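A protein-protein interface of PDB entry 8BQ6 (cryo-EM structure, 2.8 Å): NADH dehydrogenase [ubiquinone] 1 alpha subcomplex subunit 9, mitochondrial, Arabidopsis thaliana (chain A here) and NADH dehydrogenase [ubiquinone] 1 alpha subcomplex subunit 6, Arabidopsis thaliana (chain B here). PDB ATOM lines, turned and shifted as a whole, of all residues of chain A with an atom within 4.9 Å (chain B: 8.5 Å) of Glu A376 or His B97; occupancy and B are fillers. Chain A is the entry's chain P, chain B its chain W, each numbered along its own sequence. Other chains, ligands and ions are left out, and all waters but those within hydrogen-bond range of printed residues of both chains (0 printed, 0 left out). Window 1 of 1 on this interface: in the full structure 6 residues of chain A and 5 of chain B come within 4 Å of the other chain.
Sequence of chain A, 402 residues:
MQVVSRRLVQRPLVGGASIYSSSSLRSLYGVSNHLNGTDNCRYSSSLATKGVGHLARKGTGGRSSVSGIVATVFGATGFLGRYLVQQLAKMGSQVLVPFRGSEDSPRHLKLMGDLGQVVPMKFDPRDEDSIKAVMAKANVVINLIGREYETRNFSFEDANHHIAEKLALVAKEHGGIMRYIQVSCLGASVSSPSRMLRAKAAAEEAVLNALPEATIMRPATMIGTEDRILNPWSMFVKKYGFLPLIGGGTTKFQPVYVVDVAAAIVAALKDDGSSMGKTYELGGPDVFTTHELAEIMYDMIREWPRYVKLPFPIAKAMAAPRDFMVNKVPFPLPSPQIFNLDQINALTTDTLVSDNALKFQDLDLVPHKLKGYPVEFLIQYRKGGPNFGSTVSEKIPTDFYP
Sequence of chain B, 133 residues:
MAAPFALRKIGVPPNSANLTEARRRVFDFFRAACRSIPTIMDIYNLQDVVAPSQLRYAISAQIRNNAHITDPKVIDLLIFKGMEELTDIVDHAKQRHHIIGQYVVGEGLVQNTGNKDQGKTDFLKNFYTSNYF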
ATOM      1  N   TYR A 257     -42.846  24.768 -24.982  1.00  0.00           N
ATOM      2  CA  TYR A 257     -41.534  25.061 -24.423  1.00  0.00           C
ATOM      3  C   TYR A 257     -41.422  26.545 -24.098  1.00  0.00           C
ATOM      4  O   TYR A 257     -41.757  27.400 -24.924  1.00  0.00           O
ATOM      5  CB  TYR A 257     -40.456  24.643 -25.420  1.00  0.00           C
ATOM      6  CG  TYR A 257     -39.047  24.636 -24.882  1.00  0.00           C
ATOM      7  CD1 TYR A 257     -38.788  24.368 -23.546  1.00  0.00           C
ATOM      8  CD2 TYR A 257     -37.973  24.896 -25.719  1.00  0.00           C
ATOM      9  CE1 TYR A 257     -37.496  24.362 -23.061  1.00  0.00           C
ATOM     10  CE2 TYR A 257     -36.683  24.889 -25.247  1.00  0.00           C
ATOM     11  CZ  TYR A 257     -36.448  24.622 -23.919  1.00  0.00           C
ATOM     12  OH  TYR A 257     -35.158  24.618 -23.449  1.00  0.00           O
ATOM     13  N   MET A 300     -38.581  10.097 -18.511  1.00  0.00           N
ATOM     14  CA  MET A 300     -37.379  10.895 -18.289  1.00  0.00           C
ATOM     15  C   MET A 300     -36.779  10.644 -16.909  1.00  0.00           C
ATOM     16  O   MET A 300     -35.555  10.550 -16.770  1.00  0.00           O
ATOM     17  CB  MET A 300     -37.681  12.380 -18.488  1.00  0.00           C
ATOM     18  CG  MET A 300     -38.169  12.723 -19.887  1.00  0.00           C
ATOM     19  SD  MET A 300     -36.872  12.713 -21.140  1.00  0.00           S
ATOM     20  CE  MET A 300     -35.612  13.693 -20.333  1.00  0.00           C
ATOM     21  N   GLY A 372     -37.004  15.599 -25.583  1.00  0.00           N
ATOM     22  CA  GLY A 372     -35.637  16.018 -25.826  1.00  0.00           C
ATOM     23  C   GLY A 372     -35.127  17.020 -24.811  1.00  0.00           C
ATOM     24  O   GLY A 372     -35.332  16.844 -23.607  1.00  0.00           O
ATOM     25  N   TYR A 373     -34.453  18.077 -25.286  1.00  0.00           N
ATOM     26  CA  TYR A 373     -34.011  19.132 -24.372  1.00  0.00           C
ATOM     27  C   TYR A 373     -35.141  19.777 -23.579  1.00  0.00           C
ATOM     28  O   TYR A 373     -34.926  20.079 -22.392  1.00  0.00           O
ATOM     29  CB  TYR A 373     -33.212  20.197 -25.122  1.00  0.00           C
ATOM     30  CG  TYR A 373     -32.308  19.676 -26.194  1.00  0.00           C
ATOM     31  CD1 TYR A 373     -32.703  19.653 -27.518  1.00  0.00           C
ATOM     32  CD2 TYR A 373     -31.058  19.180 -25.869  1.00  0.00           C
ATOM     33  CE1 TYR A 373     -31.861  19.180 -28.492  1.00  0.00           C
ATOM     34  CE2 TYR A 373     -30.220  18.699 -26.825  1.00  0.00           C
ATOM     35  CZ  TYR A 373     -30.622  18.698 -28.135  1.00  0.00           C
ATOM     36  OH  TYR A 373     -29.763  18.216 -29.089  1.00  0.00           O
ATOM     37  N   PRO A 374     -36.323  20.057 -24.145  1.00  0.00           N
ATOM     38  CA  PRO A 374     -37.339  20.764 -23.345  1.00  0.00           C
ATOM     39  C   PRO A 374     -37.723  20.056 -22.058  1.00  0.00           C
ATOM     40  O   PRO A 374     -38.273  20.698 -21.156  1.00  0.00           O
ATOM     41  CB  PRO A 374     -38.529  20.879 -24.309  1.00  0.00           C
ATOM     42  CG  PRO A 374     -37.933  20.784 -25.646  1.00  0.00           C
ATOM     43  CD  PRO A 374     -36.799  19.836 -25.523  1.00  0.00           C
ATOM     44  N   VAL A 375     -37.457  18.756 -21.931  1.00  0.00           N
ATOM     45  CA  VAL A 375     -37.676  18.071 -20.664  1.00  0.00           C
ATOM     46  C   VAL A 375     -36.386  17.540 -20.065  1.00  0.00           C
ATOM     47  O   VAL A 375     -36.431  16.762 -19.103  1.00  0.00           O
ATOM     48  CB  VAL A 375     -38.706  16.935 -20.819  1.00  0.00           C
ATOM     49  CG1 VAL A 375     -40.037  17.497 -21.297  1.00  0.00           C
ATOM     50  CG2 VAL A 375     -38.193  15.880 -21.775  1.00  0.00           C
ATOM     51  N   GLU A 376     -35.231  17.963 -20.587  1.00  0.00           N
ATOM     52  CA  GLU A 376     -33.960  17.408 -20.139  1.00  0.00           C
ATOM     53  C   GLU A 376     -33.671  17.759 -18.685  1.00  0.00           C
ATOM     54  O   GLU A 376     -32.883  17.073 -18.025  1.00  0.00           O
ATOM     55  CB  GLU A 376     -32.839  17.893 -21.064  1.00  0.00           C
ATOM     56  CG  GLU A 376     -31.464  17.297 -20.800  1.00  0.00           C
ATOM     57  CD  GLU A 376     -30.342  18.175 -21.329  1.00  0.00           C
ATOM     58  OE1 GLU A 376     -29.164  17.887 -21.032  1.00  0.00           O
ATOM     59  OE2 GLU A 376     -30.641  19.149 -22.051  1.00  0.00           O
ATOM     60  N   PHE A 377     -34.322  18.799 -18.155  1.00  0.00           N
ATOM     61  CA  PHE A 377     -34.144  19.144 -16.749  1.00  0.00           C
ATOM     62  C   PHE A 377     -34.620  18.039 -15.814  1.00  0.00           C
ATOM     63  O   PHE A 377     -34.187  17.992 -14.658  1.00  0.00           O
ATOM     64  CB  PHE A 377     -34.872  20.451 -16.430  1.00  0.00           C
ATOM     65  CG  PHE A 377     -36.367  20.336 -16.452  1.00  0.00           C
ATOM     66  CD1 PHE A 377     -37.060  20.402 -17.647  1.00  0.00           C
ATOM     67  CD2 PHE A 377     -37.080  20.161 -15.280  1.00  0.00           C
ATOM     68  CE1 PHE A 377     -38.432  20.299 -17.671  1.00  0.00           C
ATOM     69  CE2 PHE A 377     -38.450  20.057 -15.300  1.00  0.00           C
ATOM     70  CZ  PHE A 377     -39.128  20.124 -16.496  1.00  0.00           C
ATOM     71  N   LEU A 378     -35.483  17.141 -16.291  1.00  0.00           N
ATOM     72  CA  LEU A 378     -35.988  16.045 -15.474  1.00  0.00           C
ATOM     73  C   LEU A 378     -34.916  15.019 -15.143  1.00  0.00           C
ATOM     74  O   LEU A 378     -35.176  14.104 -14.354  1.00  0.00           O
ATOM     75  CB  LEU A 378     -37.150  15.370 -16.191  1.00  0.00           C
ATOM     76  CG  LEU A 378     -38.374  16.261 -16.372  1.00  0.00           C
ATOM     77  CD1 LEU A 378     -39.383  15.557 -17.244  1.00  0.00           C
ATOM     78  CD2 LEU A 378     -38.974  16.600 -15.024  1.00  0.00           C
ATOM     79  N   ILE A 379     -33.732  15.145 -15.743  1.00  0.00           N
ATOM     80  CA  ILE A 379     -32.610  14.274 -15.422  1.00  0.00           C
ATOM     81  C   ILE A 379     -32.249  14.379 -13.946  1.00  0.00           C
ATOM     82  O   ILE A 379     -31.840  13.389 -13.325  1.00  0.00           O
ATOM     83  CB  ILE A 379     -31.414  14.628 -16.334  1.00  0.00           C
ATOM     84  CG1 ILE A 379     -31.715  14.307 -17.805  1.00  0.00           C
ATOM     85  CG2 ILE A 379     -30.127  13.960 -15.863  1.00  0.00           C
ATOM     86  CD1 ILE A 379     -30.713  14.859 -18.791  1.00  0.00           C
ATOM     87  N   ASP B  42     -25.430   8.397 -25.065  1.00  0.00           N
ATOM     88  CA  ASP B  42     -25.745   8.377 -23.642  1.00  0.00           C
ATOM     89  C   ASP B  42     -25.272   9.655 -22.954  1.00  0.00           C
ATOM     90  O   ASP B  42     -25.981  10.214 -22.109  1.00  0.00           O
ATOM     91  CB  ASP B  42     -25.121   7.139 -22.997  1.00  0.00           C
ATOM     92  CG  ASP B  42     -25.722   6.819 -21.644  1.00  0.00           C
ATOM     93  OD1 ASP B  42     -26.106   7.757 -20.920  1.00  0.00           O
ATOM     94  OD2 ASP B  42     -25.812   5.620 -21.301  1.00  0.00           O
ATOM     95  N   ILE B  43     -24.057  10.117 -23.259  1.00  0.00           N
ATOM     96  CA  ILE B  43     -23.499  11.314 -22.556  1.00  0.00           C
ATOM     97  C   ILE B  43     -24.351  12.551 -22.868  1.00  0.00           C
ATOM     98  O   ILE B  43     -24.702  13.270 -21.916  1.00  0.00           O
ATOM     99  CB  ILE B  43     -22.012  11.523 -22.920  1.00  0.00           C
ATOM    100  CG1 ILE B  43     -21.141  10.354 -22.456  1.00  0.00           C
ATOM    101  CG2 ILE B  43     -21.491  12.840 -22.373  1.00  0.00           C
ATOM    102  CD1 ILE B  43     -19.837  10.241 -23.204  1.00  0.00           C
ATOM    103  N   TYR B  44     -24.712  12.775 -24.131  1.00  0.00           N
ATOM    104  CA  TYR B  44     -25.425  13.991 -24.498  1.00  0.00           C
ATOM    105  C   TYR B  44     -26.942  13.820 -24.517  1.00  0.00           C
ATOM    106  O   TYR B  44     -27.646  14.771 -24.871  1.00  0.00           O
ATOM    107  CB  TYR B  44     -24.944  14.494 -25.865  1.00  0.00           C
ATOM    108  CG  TYR B  44     -23.481  14.894 -25.911  1.00  0.00           C
ATOM    109  CD1 TYR B  44     -22.482  13.935 -25.988  1.00  0.00           C
ATOM    110  CD2 TYR B  44     -23.104  16.231 -25.901  1.00  0.00           C
ATOM    111  CE1 TYR B  44     -21.149  14.290 -26.036  1.00  0.00           C
ATOM    112  CE2 TYR B  44     -21.770  16.596 -25.952  1.00  0.00           C
ATOM    113  CZ  TYR B  44     -20.798  15.621 -26.019  1.00  0.00           C
ATOM    114  OH  TYR B  44     -19.470  15.973 -26.069  1.00  0.00           O
ATOM    115  N   ASN B  45     -27.455  12.647 -24.147  1.00  0.00           N
ATOM    116  CA  ASN B  45     -28.893  12.377 -24.081  1.00  0.00           C
ATOM    117  C   ASN B  45     -29.579  12.739 -25.401  1.00  0.00           C
ATOM    118  O   ASN B  45     -30.459  13.596 -25.472  1.00  0.00           O
ATOM    119  CB  ASN B  45     -29.538  13.138 -22.919  1.00  0.00           C
ATOM    120  CG  ASN B  45     -28.719  13.069 -21.652  1.00  0.00           C
ATOM    121  OD1 ASN B  45     -28.594  12.012 -21.035  1.00  0.00           O
ATOM    122  ND2 ASN B  45     -28.145  14.200 -21.260  1.00  0.00           N
ATOM    123  N   LEU B  46     -29.139  12.061 -26.457  1.00  0.00           N
ATOM    124  CA  LEU B  46     -29.590  12.369 -27.807  1.00  0.00           C
ATOM    125  C   LEU B  46     -30.658  11.406 -28.308  1.00  0.00           C
ATOM    126  O   LEU B  46     -30.956  11.402 -29.506  1.00  0.00           O
ATOM    127  CB  LEU B  46     -28.401  12.383 -28.769  1.00  0.00           C
ATOM    128  CG  LEU B  46     -27.172  13.173 -28.319  1.00  0.00           C
ATOM    129  CD1 LEU B  46     -25.913  12.591 -28.930  1.00  0.00           C
ATOM    130  CD2 LEU B  46     -27.318  14.637 -28.692  1.00  0.00           C
ATOM    131  N   GLN B  47     -31.250  10.606 -27.417  1.00  0.00           N
ATOM    132  CA  GLN B  47     -32.178   9.561 -27.842  1.00  0.00           C
ATOM    133  C   GLN B  47     -33.378  10.134 -28.585  1.00  0.00           C
ATOM    134  O   GLN B  47     -33.951   9.472 -29.459  1.00  0.00           O
ATOM    135  CB  GLN B  47     -32.639   8.748 -26.630  1.00  0.00           C
ATOM    136  CG  GLN B  47     -31.527   7.964 -25.945  1.00  0.00           C
ATOM    137  CD  GLN B  47     -30.645   8.831 -25.064  1.00  0.00           C
ATOM    138  OE1 GLN B  47     -31.082   9.859 -24.548  1.00  0.00           O
ATOM    139  NE2 GLN B  47     -29.396   8.419 -24.891  1.00  0.00           N
ATOM    140  N   ASP B  48     -33.772  11.364 -28.259  1.00  0.00           N
ATOM    141  CA  ASP B  48     -34.918  12.006 -28.886  1.00  0.00           C
ATOM    142  C   ASP B  48     -34.517  13.182 -29.764  1.00  0.00           C
ATOM    143  O   ASP B  48     -35.365  14.014 -30.103  1.00  0.00           O
ATOM    144  CB  ASP B  48     -35.912  12.452 -27.818  1.00  0.00           C
ATOM    145  CG  ASP B  48     -36.324  11.317 -26.912  1.00  0.00           C
ATOM    146  OD1 ASP B  48     -36.163  10.151 -27.327  1.00  0.00           O
ATOM    147  OD2 ASP B  48     -36.801  11.581 -25.791  1.00  0.00           O
ATOM    148  N   VAL B  49     -33.242  13.268 -30.141  1.00  0.00           N
ATOM    149  CA  VAL B  49     -32.723  14.394 -30.900  1.00  0.00           C
ATOM    150  C   VAL B  49     -32.242  13.976 -32.282  1.00  0.00           C
ATOM    151  O   VAL B  49     -32.549  14.642 -33.279  1.00  0.00           O
ATOM    152  CB  VAL B  49     -31.590  15.101 -30.131  1.00  0.00           C
ATOM    153  CG1 VAL B  49     -30.947  16.159 -31.006  1.00  0.00           C
ATOM    154  CG2 VAL B  49     -32.120  15.699 -28.837  1.00  0.00           C
ATOM    155  N   LYS B  94     -18.467  18.910 -23.540  1.00  0.00           N
ATOM    156  CA  LYS B  94     -18.916  20.291 -23.391  1.00  0.00           C
ATOM    157  C   LYS B  94     -20.301  20.363 -24.020  1.00  0.00           C
ATOM    158  O   LYS B  94     -20.451  20.598 -25.220  1.00  0.00           O
ATOM    159  CB  LYS B  94     -17.947  21.271 -24.021  1.00  0.00           C
ATOM    160  CG  LYS B  94     -16.877  21.712 -23.056  1.00  0.00           C
ATOM    161  CD  LYS B  94     -15.768  22.453 -23.749  1.00  0.00           C
ATOM    162  CE  LYS B  94     -14.435  21.972 -23.236  1.00  0.00           C
ATOM    163  NZ  LYS B  94     -14.525  21.407 -21.870  1.00  0.00           N
ATOM    164  N   GLN B  95     -21.312  20.157 -23.186  1.00  0.00           N
ATOM    165  CA  GLN B  95     -22.662  19.971 -23.684  1.00  0.00           C
ATOM    166  C   GLN B  95     -23.245  21.295 -24.154  1.00  0.00           C
ATOM    167  O   GLN B  95     -23.181  22.306 -23.452  1.00  0.00           O
ATOM    168  CB  GLN B  95     -23.524  19.344 -22.593  1.00  0.00           C
ATOM    169  CG  GLN B  95     -22.949  18.024 -22.116  1.00  0.00           C
ATOM    170  CD  GLN B  95     -23.999  17.026 -21.683  1.00  0.00           C
ATOM    171  OE1 GLN B  95     -25.046  16.888 -22.314  1.00  0.00           O
ATOM    172  NE2 GLN B  95     -23.715  16.312 -20.603  1.00  0.00           N
ATOM    173  N   ARG B  96     -23.761  21.282 -25.376  1.00  0.00           N
ATOM    174  CA  ARG B  96     -24.542  22.367 -25.944  1.00  0.00           C
ATOM    175  C   ARG B  96     -25.715  21.708 -26.650  1.00  0.00           C
ATOM    176  O   ARG B  96     -25.572  20.587 -27.149  1.00  0.00           O
ATOM    177  CB  ARG B  96     -23.702  23.207 -26.902  1.00  0.00           C
ATOM    178  CG  ARG B  96     -24.323  24.530 -27.262  1.00  0.00           C
ATOM    179  CD  ARG B  96     -24.649  25.330 -26.020  1.00  0.00           C
ATOM    180  NE  ARG B  96     -25.139  26.666 -26.337  1.00  0.00           N
ATOM    181  CZ  ARG B  96     -24.434  27.602 -26.959  1.00  0.00           C
ATOM    182  NH1 ARG B  96     -23.183  27.393 -27.336  1.00  0.00           N
ATOM    183  NH2 ARG B  96     -24.995  28.784 -27.197  1.00  0.00           N
ATOM    184  N   HIS B  97     -26.868  22.374 -26.700  1.00  0.00           N
ATOM    185  CA  HIS B  97     -28.104  21.701 -27.083  1.00  0.00           C
ATOM    186  C   HIS B  97     -28.005  21.022 -28.445  1.00  0.00           C
ATOM    187  O   HIS B  97     -27.974  19.790 -28.524  1.00  0.00           O
ATOM    188  CB  HIS B  97     -29.265  22.697 -27.080  1.00  0.00           C
ATOM    189  CG  HIS B  97     -30.076  22.682 -25.821  1.00  0.00           C
ATOM    190  ND1 HIS B  97     -31.197  23.465 -25.650  1.00  0.00           N
ATOM    191  CD2 HIS B  97     -29.927  21.982 -24.671  1.00  0.00           C
ATOM    192  CE1 HIS B  97     -31.703  23.249 -24.450  1.00  0.00           C
ATOM    193  NE2 HIS B  97     -30.953  22.353 -23.835  1.00  0.00           N
ATOM    194  N   HIS B  98     -27.968  21.802 -29.515  1.00  0.00           N
ATOM    195  CA  HIS B  98     -27.972  21.156 -30.851  1.00  0.00           C
ATOM    196  C   HIS B  98     -26.547  21.102 -31.401  1.00  0.00           C
ATOM    197  O   HIS B  98     -26.410  21.176 -32.632  1.00  0.00           O
ATOM    198  CB  HIS B  98     -28.943  21.899 -31.774  1.00  0.00           C
ATOM    199  CG  HIS B  98     -30.377  21.562 -31.538  1.00  0.00           C
ATOM    200  ND1 HIS B  98     -30.983  20.464 -32.115  1.00  0.00           N
ATOM    201  CD2 HIS B  98     -31.325  22.173 -30.798  1.00  0.00           C
ATOM    202  CE1 HIS B  98     -32.245  20.415 -31.744  1.00  0.00           C
ATOM    203  NE2 HIS B  98     -32.480  21.454 -30.933  1.00  0.00           N
ATOM    204  N   ILE B  99     -25.533  20.974 -30.534  1.00  0.00           N
ATOM    205  CA  ILE B  99     -24.111  21.042 -30.994  1.00  0.00           C
ATOM    206  C   ILE B  99     -23.253  20.034 -30.226  1.00  0.00           C
ATOM    207  O   ILE B  99     -23.193  20.143 -28.984  1.00  0.00           O
ATOM    208  CB  ILE B  99     -23.550  22.474 -30.823  1.00  0.00           C
ATOM    209  CG1 ILE B  99     -24.240  23.500 -31.724  1.00  0.00           C
ATOM    210  CG2 ILE B  99     -22.042  22.498 -31.041  1.00  0.00           C
ATOM    211  CD1 ILE B  99     -24.369  24.870 -31.107  1.00  0.00           C
ATOM    212  N   ILE B 100     -22.617  19.088 -30.923  1.00  0.00           N
ATOM    213  CA  ILE B 100     -21.644  18.167 -30.261  1.00  0.00           C
ATOM    214  C   ILE B 100     -20.264  18.529 -30.812  1.00  0.00           C
ATOM    215  O   ILE B 100     -20.022  18.255 -31.999  1.00  0.00           O
ATOM    216  CB  ILE B 100     -21.979  16.688 -30.521  1.00  0.00           C
ATOM    217  CG1 ILE B 100     -23.376  16.320 -30.026  1.00  0.00           C
ATOM    218  CG2 ILE B 100     -20.924  15.776 -29.913  1.00  0.00           C
ATOM    219  CD1 ILE B 100     -23.720  14.891 -30.307  1.00  0.00           C
ATOM    220  N   TYR B 103     -20.200  19.861 -34.492  1.00  0.00           N
ATOM    221  CA  TYR B 103     -21.198  19.270 -35.423  1.00  0.00           C
ATOM    222  C   TYR B 103     -22.609  19.680 -35.007  1.00  0.00           C
ATOM    223  O   TYR B 103     -23.034  19.323 -33.893  1.00  0.00           O
ATOM    224  CB  TYR B 103     -21.007  17.752 -35.487  1.00  0.00           C
ATOM    225  CG  TYR B 103     -19.592  17.363 -35.823  1.00  0.00           C
ATOM    226  CD1 TYR B 103     -19.125  17.446 -37.124  1.00  0.00           C
ATOM    227  CD2 TYR B 103     -18.702  16.973 -34.837  1.00  0.00           C
ATOM    228  CE1 TYR B 103     -17.818  17.125 -37.442  1.00  0.00           C
ATOM    229  CE2 TYR B 103     -17.391  16.653 -35.137  1.00  0.00           C
ATOM    230  CZ  TYR B 103     -16.949  16.724 -36.445  1.00  0.00           C
ATOM    231  OH  TYR B 103     -15.661  16.406 -36.751  1.00  0.00           O
ATOM    232  N   VAL B 104     -23.294  20.439 -35.870  1.00  0.00           N
ATOM    233  CA  VAL B 104     -24.713  20.801 -35.582  1.00  0.00           C
ATOM    234  C   VAL B 104     -25.503  19.487 -35.571  1.00  0.00           C
ATOM    235  O   VAL B 104     -25.589  18.829 -36.627  1.00  0.00           O
ATOM    236  CB  VAL B 104     -25.266  21.856 -36.564  1.00  0.00           C
ATOM    237  CG1 VAL B 104     -26.744  22.150 -36.364  1.00  0.00           C
ATOM    238  CG2 VAL B 104     -24.437  23.133 -36.593  1.00  0.00           C
ATOM    239  N   VAL B 105     -26.006  19.093 -34.401  1.00  0.00           N
ATOM    240  CA  VAL B 105     -26.702  17.779 -34.277  1.00  0.00           C
ATOM    241  C   VAL B 105     -28.202  18.012 -34.106  1.00  0.00           C
ATOM    242  O   VAL B 105     -28.581  18.932 -33.362  1.00  0.00           O
ATOM    243  CB  VAL B 105     -26.077  16.949 -33.141  1.00  0.00           C
ATOM    244  CG1 VAL B 105     -27.067  16.051 -32.417  1.00  0.00           C
ATOM    245  CG2 VAL B 105     -24.894  16.145 -33.652  1.00  0.00           C
ATOM    246  N   GLY B 106     -29.018  17.226 -34.799  1.00  0.00           N
ATOM    247  CA  GLY B 106     -30.463  17.344 -34.763  1.00  0.00           C
ATOM    248  C   GLY B 106     -30.968  18.621 -35.405  1.00  0.00           C
ATOM    249  O   GLY B 106     -31.283  18.649 -36.595  1.00  0.00           O
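O of Asp B42 sits close to OD1 of Asn B45 (3.3 Å). The backbone carbonyl oxygen (O) of His B98 is in hydrogen-bond range of the backbone NH (N) of Val B105.
Among the printed residues, pairs that only touch across the chains: Tyr A373 with Val B49 (3.1 Å), Tyr A373 with His B98 (3.4 Å), Ile A379 with Asn B45 (3.6 Å), Glu A376 with His B97 (3.7 Å), Glu A376 with Asn B45 (3.8 Å) and Tyr A257 with His B97 (3.8 Å).
Of the 10 printed residues of chain A, 4 touch a printed residue of chain B. Printed residues of chain A that touch a printed residue of chain B: Tyr A257, Tyr A373, Glu A376 and Ile A379. Hydrophobic or aromatic side chains of chain A within 4 Å of the printed part of chain B: Tyr A257, Tyr A373 and Ile A379. Of the 19 printed residues of chain B, 4 touch a printed residue of chain A. Among the printed residues, 7 pairs touch across the chains.
The backbone carbonyl oxygen of His B97 is in hydrogen-bond range of the side-chain hydroxyl of Tyr A373 (2.4 Å).
Of the printed residues of chain B, Tyr A257 touches His B97. Glu A376 touches two residues of chain B. Printed residues of chain B within 4 Å of Ile A379: Asn B45 (3.6 Å). Printed residues of chain A within 4 Å of Val B49: Tyr A373 (3.1 Å). His B97 touches three residues of chain A. Of the printed residues of chain A, His B98 touches Tyr A373. Ile B99 touches none of the printed residues of chain A. The nearest residue of chain B that does not touch Glu A376 is Gln B95 (4.4 Å).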
